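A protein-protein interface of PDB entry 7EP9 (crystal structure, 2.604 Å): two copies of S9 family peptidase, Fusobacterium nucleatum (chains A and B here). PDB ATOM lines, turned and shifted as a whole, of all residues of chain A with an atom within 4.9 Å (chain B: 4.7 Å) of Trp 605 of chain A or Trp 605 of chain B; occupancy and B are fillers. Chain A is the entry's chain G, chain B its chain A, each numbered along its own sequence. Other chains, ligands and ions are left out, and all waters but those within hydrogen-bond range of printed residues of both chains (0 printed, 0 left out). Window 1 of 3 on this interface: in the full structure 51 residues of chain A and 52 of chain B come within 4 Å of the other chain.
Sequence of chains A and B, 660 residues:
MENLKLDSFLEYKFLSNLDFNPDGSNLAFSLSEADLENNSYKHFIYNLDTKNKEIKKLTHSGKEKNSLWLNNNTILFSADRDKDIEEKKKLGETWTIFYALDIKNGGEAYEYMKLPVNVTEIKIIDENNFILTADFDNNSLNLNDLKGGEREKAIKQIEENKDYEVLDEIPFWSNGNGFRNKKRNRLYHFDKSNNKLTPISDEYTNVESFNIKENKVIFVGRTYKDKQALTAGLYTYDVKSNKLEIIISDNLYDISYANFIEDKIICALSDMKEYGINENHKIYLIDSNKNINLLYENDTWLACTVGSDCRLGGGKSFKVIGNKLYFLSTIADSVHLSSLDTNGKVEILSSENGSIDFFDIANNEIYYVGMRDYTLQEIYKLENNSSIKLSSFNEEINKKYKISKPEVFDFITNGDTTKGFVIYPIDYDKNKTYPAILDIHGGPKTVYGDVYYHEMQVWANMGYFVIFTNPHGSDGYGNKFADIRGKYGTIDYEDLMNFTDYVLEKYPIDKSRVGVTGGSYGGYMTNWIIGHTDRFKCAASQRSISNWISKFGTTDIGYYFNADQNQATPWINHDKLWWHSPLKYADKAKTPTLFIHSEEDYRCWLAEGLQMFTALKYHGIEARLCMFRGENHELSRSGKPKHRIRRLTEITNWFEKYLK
O of Trp 605 of chain A sits at hydrogen-bond distance from NE2 of His 597 of chain A (2.9 Å). The backbone NH (N) of Leu 606 of chain A lies close to a ring nitrogen (NE2) of His 597 of chain A (3.4 Å). NE2 of His 597 of chain B sits at hydrogen-bond distance from O of Trp 605 of chain B (2.9 Å). The backbone NH of Leu 606 of chain B sits close to a ring nitrogen (NE2) of His 597 of chain B (3.4 Å).
Among the printed residues, pairs that only touch across the chains: Trp 605 of chain A with Ala 607 of chain B (3.4 Å), Trp 605 of chain A with Trp 605 of chain B (3.4 Å), Thr 554 of chain A with Leu 610 of chain B (3.7 Å), Leu 610 of chain A with Thr 554 of chain B (3.7 Å), Trp 173 of chain A with Leu 610 of chain B (3.7 Å), Leu 610 of chain A with Trp 173 of chain B (3.8 Å), Leu 606 of chain A with Trp 605 of chain B (3.9 Å) and Trp 605 of chain A with Leu 606 of chain B (3.99 Å).
Of the printed residues of chain B, Trp 605 of chain A touches Trp 605, Leu 606 and Ala 607. Gly 609 of chain A touches none of the printed residues of chain B. Printed residues of chain B within 4 Å of Leu 610 of chain A: Trp 173 and Thr 554. Of the printed residues of chain A, Thr 554 of chain B touches Leu 610 (3.7 Å). Printed residues of chain A within 4 Å of Trp 605 of chain B: Trp 605 and Leu 606. Printed residues of chain A within 4 Å of Leu 606 of chain B: Trp 605. Of the printed residues of chain A, Ala 607 of chain B touches Trp 605 (3.4 Å). Of the printed residues of chain A, Leu 610 of chain B touches Trp 173 and Thr 554. The nearest printed residue of chain B that does not touch Trp 605 of chain A is Leu 610 of chain B (4.04 Å). The nearest residue of chain A that does not touch Trp 605 of chain B is Leu 610 of chain A (4.4 Å).
Of the 15 printed residues of chain A, 5 touch a printed residue of chain B. Printed residues of chain A that touch a printed residue of chain B: Trp 173, Thr 554, Trp 605, Leu 606 and Leu 610. Printed residues of chain B that touch a printed residue of chain A: Trp 173, Thr 554, Trp 605, Leu 606, Ala 607 and Leu 610. Among the printed residues, 8 pairs touch across the chains.
Trp 173 of chain A touches Leu 610 of chain B, and with the chains exchanged Leu 610 of chain A touches Trp 173 of chain B. Thr 554 of chain A touches Leu 610 of chain B, and with the chains exchanged Leu 610 of chain A touches Thr 554 of chain B. Trp 605 of chain A touches Leu 606 of chain B, and with the chains exchanged Leu 606 of chain A touches Trp 605 of chain B. Trp 605 of chain A touches Ala 607 of chain B, but with the chains exchanged Ala 607 of chain A does not touch Trp 605 of chain B (4.5 Å). 15 positions are printed for both chains. Of the 8 pairs that touch across the chains among the printed residues, 7 have their exchanged pair printed and touching as well.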
ATOM      1  N   TRP A 173      25.771  20.948  -6.585  1.00  0.00           N
ATOM      2  CA  TRP A 173      26.486  21.525  -7.713  1.00  0.00           C
ATOM      3  C   TRP A 173      25.812  22.828  -8.114  1.00  0.00           C
ATOM      4  O   TRP A 173      24.663  23.094  -7.756  1.00  0.00           O
ATOM      5  CB  TRP A 173      26.566  20.559  -8.909  1.00  0.00           C
ATOM      6  CG  TRP A 173      25.262  19.955  -9.365  1.00  0.00           C
ATOM      7  CD1 TRP A 173      24.008  20.480  -9.224  1.00  0.00           C
ATOM      8  CD2 TRP A 173      25.096  18.709 -10.056  1.00  0.00           C
ATOM      9  NE1 TRP A 173      23.075  19.636  -9.777  1.00  0.00           N
ATOM     10  CE2 TRP A 173      23.718  18.543 -10.297  1.00  0.00           C
ATOM     11  CE3 TRP A 173      25.980  17.717 -10.491  1.00  0.00           C
ATOM     12  CZ2 TRP A 173      23.203  17.423 -10.950  1.00  0.00           C
ATOM     13  CZ3 TRP A 173      25.469  16.609 -11.141  1.00  0.00           C
ATOM     14  CH2 TRP A 173      24.093  16.470 -11.364  1.00  0.00           C
ATOM     15  N   THR A 554      17.246  16.871  -9.119  1.00  0.00           N
ATOM     16  CA  THR A 554      18.468  16.824  -9.921  1.00  0.00           C
ATOM     17  C   THR A 554      18.721  18.181 -10.586  1.00  0.00           C
ATOM     18  O   THR A 554      18.797  18.285 -11.809  1.00  0.00           O
ATOM     19  CB  THR A 554      18.394  15.734 -10.992  1.00  0.00           C
ATOM     20  OG1 THR A 554      17.430  16.105 -11.984  1.00  0.00           O
ATOM     21  CG2 THR A 554      18.002  14.390 -10.391  1.00  0.00           C
ATOM     22  N   THR A 555      18.870  19.227  -9.773  1.00  0.00           N
ATOM     23  CA  THR A 555      19.111  20.564 -10.301  1.00  0.00           C
ATOM     24  C   THR A 555      19.531  21.478  -9.157  1.00  0.00           C
ATOM     25  O   THR A 555      19.043  21.332  -8.033  1.00  0.00           O
ATOM     26  CB  THR A 555      17.860  21.113 -11.011  1.00  0.00           C
ATOM     27  OG1 THR A 555      17.739  20.494 -12.299  1.00  0.00           O
ATOM     28  CG2 THR A 555      17.939  22.617 -11.201  1.00  0.00           C
ATOM     29  N   HIS A 597      21.465  19.379 -25.493  1.00  0.00           N
ATOM     30  CA  HIS A 597      21.673  19.315 -24.055  1.00  0.00           C
ATOM     31  C   HIS A 597      23.154  19.134 -23.763  1.00  0.00           C
ATOM     32  O   HIS A 597      23.883  18.498 -24.528  1.00  0.00           O
ATOM     33  CB  HIS A 597      20.863  18.182 -23.414  1.00  0.00           C
ATOM     34  CG  HIS A 597      20.325  18.523 -22.060  1.00  0.00           C
ATOM     35  ND1 HIS A 597      19.061  19.035 -21.867  1.00  0.00           N
ATOM     36  CD2 HIS A 597      20.888  18.435 -20.832  1.00  0.00           C
ATOM     37  CE1 HIS A 597      18.865  19.243 -20.577  1.00  0.00           C
ATOM     38  NE2 HIS A 597      19.958  18.887 -19.927  1.00  0.00           N
ATOM     39  N   GLU A 599      26.214  18.067 -20.806  1.00  0.00           N
ATOM     40  CA  GLU A 599      26.391  17.121 -19.707  1.00  0.00           C
ATOM     41  C   GLU A 599      26.556  17.832 -18.370  1.00  0.00           C
ATOM     42  O   GLU A 599      26.022  17.374 -17.353  1.00  0.00           O
ATOM     43  CB  GLU A 599      27.595  16.218 -19.977  1.00  0.00           C
ATOM     44  CG  GLU A 599      27.870  15.210 -18.871  1.00  0.00           C
ATOM     45  CD  GLU A 599      28.684  14.024 -19.347  1.00  0.00           C
ATOM     46  OE1 GLU A 599      29.480  14.190 -20.295  1.00  0.00           O
ATOM     47  OE2 GLU A 599      28.519  12.922 -18.781  1.00  0.00           O
ATOM     48  N   ASP A 601      25.341  20.707 -17.494  1.00  0.00           N
ATOM     49  CA  ASP A 601      24.257  21.642 -17.225  1.00  0.00           C
ATOM     50  C   ASP A 601      23.550  21.222 -15.944  1.00  0.00           C
ATOM     51  O   ASP A 601      22.991  20.123 -15.866  1.00  0.00           O
ATOM     52  CB  ASP A 601      23.280  21.677 -18.400  1.00  0.00           C
ATOM     53  CG  ASP A 601      22.244  22.785 -18.276  1.00  0.00           C
ATOM     54  OD1 ASP A 601      22.124  23.391 -17.191  1.00  0.00           O
ATOM     55  OD2 ASP A 601      21.541  23.049 -19.274  1.00  0.00           O
ATOM     56  N   TYR A 602      23.575  22.094 -14.938  1.00  0.00           N
ATOM     57  CA  TYR A 602      22.962  21.810 -13.649  1.00  0.00           C
ATOM     58  C   TYR A 602      21.753  22.690 -13.365  1.00  0.00           C
ATOM     59  O   TYR A 602      21.152  22.569 -12.292  1.00  0.00           O
ATOM     60  CB  TYR A 602      24.004  21.953 -12.535  1.00  0.00           C
ATOM     61  CG  TYR A 602      25.238  21.110 -12.782  1.00  0.00           C
ATOM     62  CD1 TYR A 602      25.132  19.839 -13.335  1.00  0.00           C
ATOM     63  CD2 TYR A 602      26.507  21.587 -12.477  1.00  0.00           C
ATOM     64  CE1 TYR A 602      26.251  19.067 -13.574  1.00  0.00           C
ATOM     65  CE2 TYR A 602      27.633  20.818 -12.712  1.00  0.00           C
ATOM     66  CZ  TYR A 602      27.498  19.558 -13.260  1.00  0.00           C
ATOM     67  OH  TYR A 602      28.613  18.786 -13.495  1.00  0.00           O
ATOM     68  N   ARG A 603      21.384  23.567 -14.298  1.00  0.00           N
ATOM     69  CA  ARG A 603      20.137  24.317 -14.231  1.00  0.00           C
ATOM     70  C   ARG A 603      18.977  23.524 -14.817  1.00  0.00           C
ATOM     71  O   ARG A 603      17.865  23.552 -14.278  1.00  0.00           O
ATOM     72  CB  ARG A 603      20.291  25.652 -14.967  1.00  0.00           C
ATOM     73  CG  ARG A 603      19.062  26.543 -14.932  1.00  0.00           C
ATOM     74  CD  ARG A 603      18.789  27.066 -13.532  1.00  0.00           C
ATOM     75  NE  ARG A 603      20.014  27.284 -12.766  1.00  0.00           N
ATOM     76  CZ  ARG A 603      20.769  28.374 -12.850  1.00  0.00           C
ATOM     77  NH1 ARG A 603      20.428  29.359 -13.671  1.00  0.00           N
ATOM     78  NH2 ARG A 603      21.866  28.481 -12.113  1.00  0.00           N
ATOM     79  N   CYS A 604      19.222  22.819 -15.922  1.00  0.00           N
ATOM     80  CA  CYS A 604      18.286  21.864 -16.511  1.00  0.00           C
ATOM     81  C   CYS A 604      19.119  20.628 -16.836  1.00  0.00           C
ATOM     82  O   CYS A 604      19.745  20.548 -17.897  1.00  0.00           O
ATOM     83  CB  CYS A 604      17.594  22.437 -17.744  1.00  0.00           C
ATOM     84  SG  CYS A 604      16.728  23.997 -17.449  1.00  0.00           S
ATOM     85  N   TRP A 605      19.131  19.671 -15.913  1.00  0.00           N
ATOM     86  CA  TRP A 605      20.074  18.565 -15.972  1.00  0.00           C
ATOM     87  C   TRP A 605      19.708  17.594 -17.098  1.00  0.00           C
ATOM     88  O   TRP A 605      18.613  17.634 -17.669  1.00  0.00           O
ATOM     89  CB  TRP A 605      20.128  17.856 -14.619  1.00  0.00           C
ATOM     90  CG  TRP A 605      21.160  16.780 -14.524  1.00  0.00           C
ATOM     91  CD1 TRP A 605      22.508  16.912 -14.696  1.00  0.00           C
ATOM     92  CD2 TRP A 605      20.925  15.401 -14.238  1.00  0.00           C
ATOM     93  NE1 TRP A 605      23.126  15.696 -14.532  1.00  0.00           N
ATOM     94  CE2 TRP A 605      22.174  14.751 -14.250  1.00  0.00           C
ATOM     95  CE3 TRP A 605      19.779  14.652 -13.971  1.00  0.00           C
ATOM     96  CZ2 TRP A 605      22.306  13.387 -14.004  1.00  0.00           C
ATOM     97  CZ3 TRP A 605      19.911  13.303 -13.729  1.00  0.00           C
ATOM     98  CH2 TRP A 605      21.164  12.682 -13.748  1.00  0.00           C
ATOM     99  N   LEU A 606      20.658  16.702 -17.403  1.00  0.00           N
ATOM    100  CA  LEU A 606      20.577  15.850 -18.587  1.00  0.00           C
ATOM    101  C   LEU A 606      19.323  14.981 -18.603  1.00  0.00           C
ATOM    102  O   LEU A 606      18.862  14.586 -19.680  1.00  0.00           O
ATOM    103  CB  LEU A 606      21.831  14.976 -18.670  1.00  0.00           C
ATOM    104  CG  LEU A 606      21.940  13.937 -19.788  1.00  0.00           C
ATOM    105  CD1 LEU A 606      21.866  14.603 -21.151  1.00  0.00           C
ATOM    106  CD2 LEU A 606      23.225  13.133 -19.648  1.00  0.00           C
ATOM    107  N   ALA A 607      18.756  14.676 -17.432  1.00  0.00           N
ATOM    108  CA  ALA A 607      17.593  13.793 -17.383  1.00  0.00           C
ATOM    109  C   ALA A 607      16.425  14.359 -18.181  1.00  0.00           C
ATOM    110  O   ALA A 607      15.681  13.608 -18.822  1.00  0.00           O
ATOM    111  CB  ALA A 607      17.174  13.548 -15.933  1.00  0.00           C
ATOM    112  N   GLU A 608      16.251  15.683 -18.158  1.00  0.00           N
ATOM    113  CA  GLU A 608      15.124  16.295 -18.855  1.00  0.00           C
ATOM    114  C   GLU A 608      15.202  16.055 -20.358  1.00  0.00           C
ATOM    115  O   GLU A 608      14.197  15.717 -20.993  1.00  0.00           O
ATOM    116  CB  GLU A 608      15.072  17.792 -18.554  1.00  0.00           C
ATOM    117  CG  GLU A 608      15.092  18.125 -17.073  1.00  0.00           C
ATOM    118  CD  GLU A 608      14.098  17.300 -16.281  1.00  0.00           C
ATOM    119  OE1 GLU A 608      12.886  17.397 -16.563  1.00  0.00           O
ATOM    120  OE2 GLU A 608      14.531  16.553 -15.378  1.00  0.00           O
ATOM    121  N   GLY A 609      16.390  16.219 -20.943  1.00  0.00           N
ATOM    122  CA  GLY A 609      16.523  16.036 -22.379  1.00  0.00           C
ATOM    123  C   GLY A 609      16.372  14.589 -22.808  1.00  0.00           C
ATOM    124  O   GLY A 609      15.813  14.303 -23.870  1.00  0.00           O
ATOM    125  N   LEU A 610      16.862  13.656 -21.988  1.00  0.00           N
ATOM    126  CA  LEU A 610      16.802  12.244 -22.354  1.00  0.00           C
ATOM    127  C   LEU A 610      15.369  11.727 -22.355  1.00  0.00           C
ATOM    128  O   LEU A 610      14.997  10.913 -23.210  1.00  0.00           O
ATOM    129  CB  LEU A 610      17.663  11.416 -21.401  1.00  0.00           C
ATOM    130  CG  LEU A 610      19.182  11.561 -21.510  1.00  0.00           C
ATOM    131  CD1 LEU A 610      19.875  10.674 -20.486  1.00  0.00           C
ATOM    132  CD2 LEU A 610      19.656  11.232 -22.916  1.00  0.00           C
ATOM    133  N   TRP B 173      22.535   3.547 -25.215  1.00  0.00           N
ATOM    134  CA  TRP B 173      23.710   3.063 -24.506  1.00  0.00           C
ATOM    135  C   TRP B 173      23.370   1.728 -23.864  1.00  0.00           C
ATOM    136  O   TRP B 173      22.200   1.357 -23.742  1.00  0.00           O
ATOM    137  CB  TRP B 173      24.207   4.068 -23.456  1.00  0.00           C
ATOM    138  CG  TRP B 173      23.164   4.569 -22.489  1.00  0.00           C
ATOM    139  CD1 TRP B 173      22.044   3.912 -22.064  1.00  0.00           C
ATOM    140  CD2 TRP B 173      23.160   5.836 -21.819  1.00  0.00           C
ATOM    141  NE1 TRP B 173      21.344   4.692 -21.178  1.00  0.00           N
ATOM    142  CE2 TRP B 173      22.009   5.878 -21.009  1.00  0.00           C
ATOM    143  CE3 TRP B 173      24.019   6.940 -21.828  1.00  0.00           C
ATOM    144  CZ2 TRP B 173      21.693   6.982 -20.218  1.00  0.00           C
ATOM    145  CZ3 TRP B 173      23.704   8.032 -21.041  1.00  0.00           C
ATOM    146  CH2 TRP B 173      22.552   8.045 -20.247  1.00  0.00           C
ATOM    147  N   THR B 554      15.552   7.020 -19.366  1.00  0.00           N
ATOM    148  CA  THR B 554      16.997   7.178 -19.241  1.00  0.00           C
ATOM    149  C   THR B 554      17.720   5.860 -18.971  1.00  0.00           C
ATOM    150  O   THR B 554      18.862   5.882 -18.495  1.00  0.00           O
ATOM    151  CB  THR B 554      17.354   8.167 -18.121  1.00  0.00           C
ATOM    152  OG1 THR B 554      16.947   7.626 -16.857  1.00  0.00           O
ATOM    153  CG2 THR B 554      16.680   9.517 -18.336  1.00  0.00           C
ATOM    154  N   THR B 555      17.101   4.719 -19.260  1.00  0.00           N
ATOM    155  CA  THR B 555      17.668   3.419 -18.931  1.00  0.00           C
ATOM    156  C   THR B 555      17.790   2.572 -20.192  1.00  0.00           C
ATOM    157  O   THR B 555      16.928   2.627 -21.075  1.00  0.00           O
ATOM    158  CB  THR B 555      16.804   2.703 -17.882  1.00  0.00           C
ATOM    159  OG1 THR B 555      16.842   3.438 -16.652  1.00  0.00           O
ATOM    160  CG2 THR B 555      17.301   1.288 -17.630  1.00  0.00           C
ATOM    161  N   HIS B 597      26.176   5.096  -6.091  1.00  0.00           N
ATOM    162  CA  HIS B 597      25.761   5.120  -7.486  1.00  0.00           C
ATOM    163  C   HIS B 597      26.959   5.423  -8.373  1.00  0.00           C
ATOM    164  O   HIS B 597      27.891   6.122  -7.968  1.00  0.00           O
ATOM    165  CB  HIS B 597      24.647   6.142  -7.730  1.00  0.00           C
ATOM    166  CG  HIS B 597      23.731   5.766  -8.850  1.00  0.00           C
ATOM    167  ND1 HIS B 597      22.548   5.090  -8.649  1.00  0.00           N
ATOM    168  CD2 HIS B 597      23.837   5.949 -10.188  1.00  0.00           C
ATOM    169  CE1 HIS B 597      21.958   4.884  -9.813  1.00  0.00           C
ATOM    170  NE2 HIS B 597      22.720   5.395 -10.762  1.00  0.00           N
ATOM    171  N   GLU B 599      28.406   6.768 -12.233  1.00  0.00           N
ATOM    172  CA  GLU B 599      28.030   7.744 -13.251  1.00  0.00           C
ATOM    173  C   GLU B 599      27.711   7.083 -14.586  1.00  0.00           C
ATOM    174  O   GLU B 599      26.828   7.555 -15.313  1.00  0.00           O
ATOM    175  CB  GLU B 599      29.142   8.777 -13.424  1.00  0.00           C
ATOM    176  CG  GLU B 599      28.733  10.001 -14.227  1.00  0.00           C
ATOM    177  CD  GLU B 599      29.734  11.133 -14.117  1.00  0.00           C
ATOM    178  OE1 GLU B 599      30.950  10.853 -14.077  1.00  0.00           O
ATOM    179  OE2 GLU B 599      29.304  12.306 -14.070  1.00  0.00           O
ATOM    180  N   ASP B 601      26.537   4.020 -14.880  1.00  0.00           N
ATOM    181  CA  ASP B 601      25.512   3.001 -14.686  1.00  0.00           C
ATOM    182  C   ASP B 601      24.301   3.355 -15.539  1.00  0.00           C
ATOM    183  O   ASP B 601      23.600   4.334 -15.262  1.00  0.00           O
ATOM    184  CB  ASP B 601      25.136   2.904 -13.210  1.00  0.00           C
ATOM    185  CG  ASP B 601      24.197   1.743 -12.913  1.00  0.00           C
ATOM    186  OD1 ASP B 601      23.673   1.119 -13.859  1.00  0.00           O
ATOM    187  OD2 ASP B 601      23.980   1.453 -11.719  1.00  0.00           O
ATOM    188  N   TYR B 602      24.051   2.560 -16.577  1.00  0.00           N
ATOM    189  CA  TYR B 602      22.935   2.790 -17.480  1.00  0.00           C
ATOM    190  C   TYR B 602      21.804   1.794 -17.281  1.00  0.00           C
ATOM    191  O   TYR B 602      20.757   1.926 -17.926  1.00  0.00           O
ATOM    192  CB  TYR B 602      23.429   2.767 -18.931  1.00  0.00           C
ATOM    193  CG  TYR B 602      24.553   3.751 -19.164  1.00  0.00           C
ATOM    194  CD1 TYR B 602      24.457   5.059 -18.706  1.00  0.00           C
ATOM    195  CD2 TYR B 602      25.716   3.371 -19.820  1.00  0.00           C
ATOM    196  CE1 TYR B 602      25.480   5.963 -18.903  1.00  0.00           C
ATOM    197  CE2 TYR B 602      26.748   4.271 -20.024  1.00  0.00           C
ATOM    198  CZ  TYR B 602      26.622   5.567 -19.564  1.00  0.00           C
ATOM    199  OH  TYR B 602      27.641   6.469 -19.761  1.00  0.00           O
ATOM    200  N   ARG B 603      21.985   0.802 -16.408  1.00  0.00           N
ATOM    201  CA  ARG B 603      20.869  -0.032 -15.976  1.00  0.00           C
ATOM    202  C   ARG B 603      20.007   0.700 -14.957  1.00  0.00           C
ATOM    203  O   ARG B 603      18.783   0.532 -14.933  1.00  0.00           O
ATOM    204  CB  ARG B 603      21.389  -1.345 -15.394  1.00  0.00           C
ATOM    205  CG  ARG B 603      20.305  -2.357 -15.075  1.00  0.00           C
ATOM    206  CD  ARG B 603      19.595  -2.811 -16.337  1.00  0.00           C
ATOM    207  NE  ARG B 603      20.529  -3.059 -17.432  1.00  0.00           N
ATOM    208  CZ  ARG B 603      21.234  -4.177 -17.576  1.00  0.00           C
ATOM    209  NH1 ARG B 603      21.114  -5.159 -16.694  1.00  0.00           N
ATOM    210  NH2 ARG B 603      22.060  -4.313 -18.604  1.00  0.00           N
ATOM    211  N   CYS B 604      20.634   1.509 -14.103  1.00  0.00           N
ATOM    212  CA  CYS B 604      19.926   2.391 -13.177  1.00  0.00           C
ATOM    213  C   CYS B 604      20.638   3.738 -13.237  1.00  0.00           C
ATOM    214  O   CYS B 604      21.718   3.904 -12.662  1.00  0.00           O
ATOM    215  CB  CYS B 604      19.899   1.821 -11.764  1.00  0.00           C
ATOM    216  SG  CYS B 604      18.939   0.294 -11.611  1.00  0.00           S
ATOM    217  N   TRP B 605      20.030   4.687 -13.944  1.00  0.00           N
ATOM    218  CA  TRP B 605      20.664   5.960 -14.249  1.00  0.00           C
ATOM    219  C   TRP B 605      20.926   6.759 -12.972  1.00  0.00           C
ATOM    220  O   TRP B 605      20.307   6.541 -11.927  1.00  0.00           O
ATOM    221  CB  TRP B 605      19.783   6.745 -15.226  1.00  0.00           C
ATOM    222  CG  TRP B 605      20.266   8.113 -15.628  1.00  0.00           C
ATOM    223  CD1 TRP B 605      19.524   9.258 -15.653  1.00  0.00           C
ATOM    224  CD2 TRP B 605      21.574   8.475 -16.094  1.00  0.00           C
ATOM    225  NE1 TRP B 605      20.289  10.312 -16.088  1.00  0.00           N
ATOM    226  CE2 TRP B 605      21.550   9.859 -16.366  1.00  0.00           C
ATOM    227  CE3 TRP B 605      22.764   7.769 -16.298  1.00  0.00           C
ATOM    228  CZ2 TRP B 605      22.668  10.548 -16.832  1.00  0.00           C
ATOM    229  CZ3 TRP B 605      23.873   8.455 -16.760  1.00  0.00           C
ATOM    230  CH2 TRP B 605      23.817   9.831 -17.021  1.00  0.00           C
ATOM    231  N   LEU B 606      21.877   7.694 -13.071  1.00  0.00           N
ATOM    232  CA  LEU B 606      22.270   8.500 -11.918  1.00  0.00           C
ATOM    233  C   LEU B 606      21.106   9.316 -11.368  1.00  0.00           C
ATOM    234  O   LEU B 606      21.094   9.654 -10.178  1.00  0.00           O
ATOM    235  CB  LEU B 606      23.430   9.420 -12.302  1.00  0.00           C
ATOM    236  CG  LEU B 606      24.026  10.340 -11.234  1.00  0.00           C
ATOM    237  CD1 LEU B 606      24.725   9.540 -10.145  1.00  0.00           C
ATOM    238  CD2 LEU B 606      24.983  11.334 -11.871  1.00  0.00           C
ATOM    239  N   ALA B 607      20.118   9.631 -12.212  1.00  0.00           N
ATOM    240  CA  ALA B 607      18.967  10.412 -11.765  1.00  0.00           C
ATOM    241  C   ALA B 607      18.238   9.744 -10.608  1.00  0.00           C
ATOM    242  O   ALA B 607      17.687  10.433  -9.742  1.00  0.00           O
ATOM    243  CB  ALA B 607      17.998  10.634 -12.927  1.00  0.00           C
ATOM    244  N   GLU B 608      18.220   8.410 -10.578  1.00  0.00           N
ATOM    245  CA  GLU B 608      17.472   7.702  -9.545  1.00  0.00           C
ATOM    246  C   GLU B 608      18.065   7.955  -8.164  1.00  0.00           C
ATOM    247  O   GLU B 608      17.353   8.342  -7.231  1.00  0.00           O
ATOM    248  CB  GLU B 608      17.439   6.207  -9.859  1.00  0.00           C
ATOM    249  CG  GLU B 608      16.905   5.883 -11.244  1.00  0.00           C
ATOM    250  CD  GLU B 608      15.591   6.581 -11.536  1.00  0.00           C
ATOM    251  OE1 GLU B 608      14.660   6.470 -10.711  1.00  0.00           O
ATOM    252  OE2 GLU B 608      15.489   7.244 -12.588  1.00  0.00           O
ATOM    253  N   GLY B 609      19.374   7.742  -8.015  1.00  0.00           N
ATOM    254  CA  GLY B 609      20.014   8.004  -6.738  1.00  0.00           C
ATOM    255  C   GLY B 609      20.025   9.471  -6.365  1.00  0.00           C
ATOM    256  O   GLY B 609      19.958   9.814  -5.181  1.00  0.00           O
ATOM    257  N   LEU B 610      20.102  10.357  -7.362  1.00  0.00           N
ATOM    258  CA  LEU B 610      20.118  11.789  -7.087  1.00  0.00           C
ATOM    259  C   LEU B 610      18.792  12.273  -6.515  1.00  0.00           C
ATOM    260  O   LEU B 610      18.765  13.251  -5.759  1.00  0.00           O
ATOM    261  CB  LEU B 610      20.448  12.568  -8.360  1.00  0.00           C
ATOM    262  CG  LEU B 610      21.912  12.663  -8.794  1.00  0.00           C
ATOM    263  CD1 LEU B 610      22.062  13.665  -9.930  1.00  0.00           C
ATOM    264  CD2 LEU B 610      22.802  13.041  -7.623  1.00  0.00           C
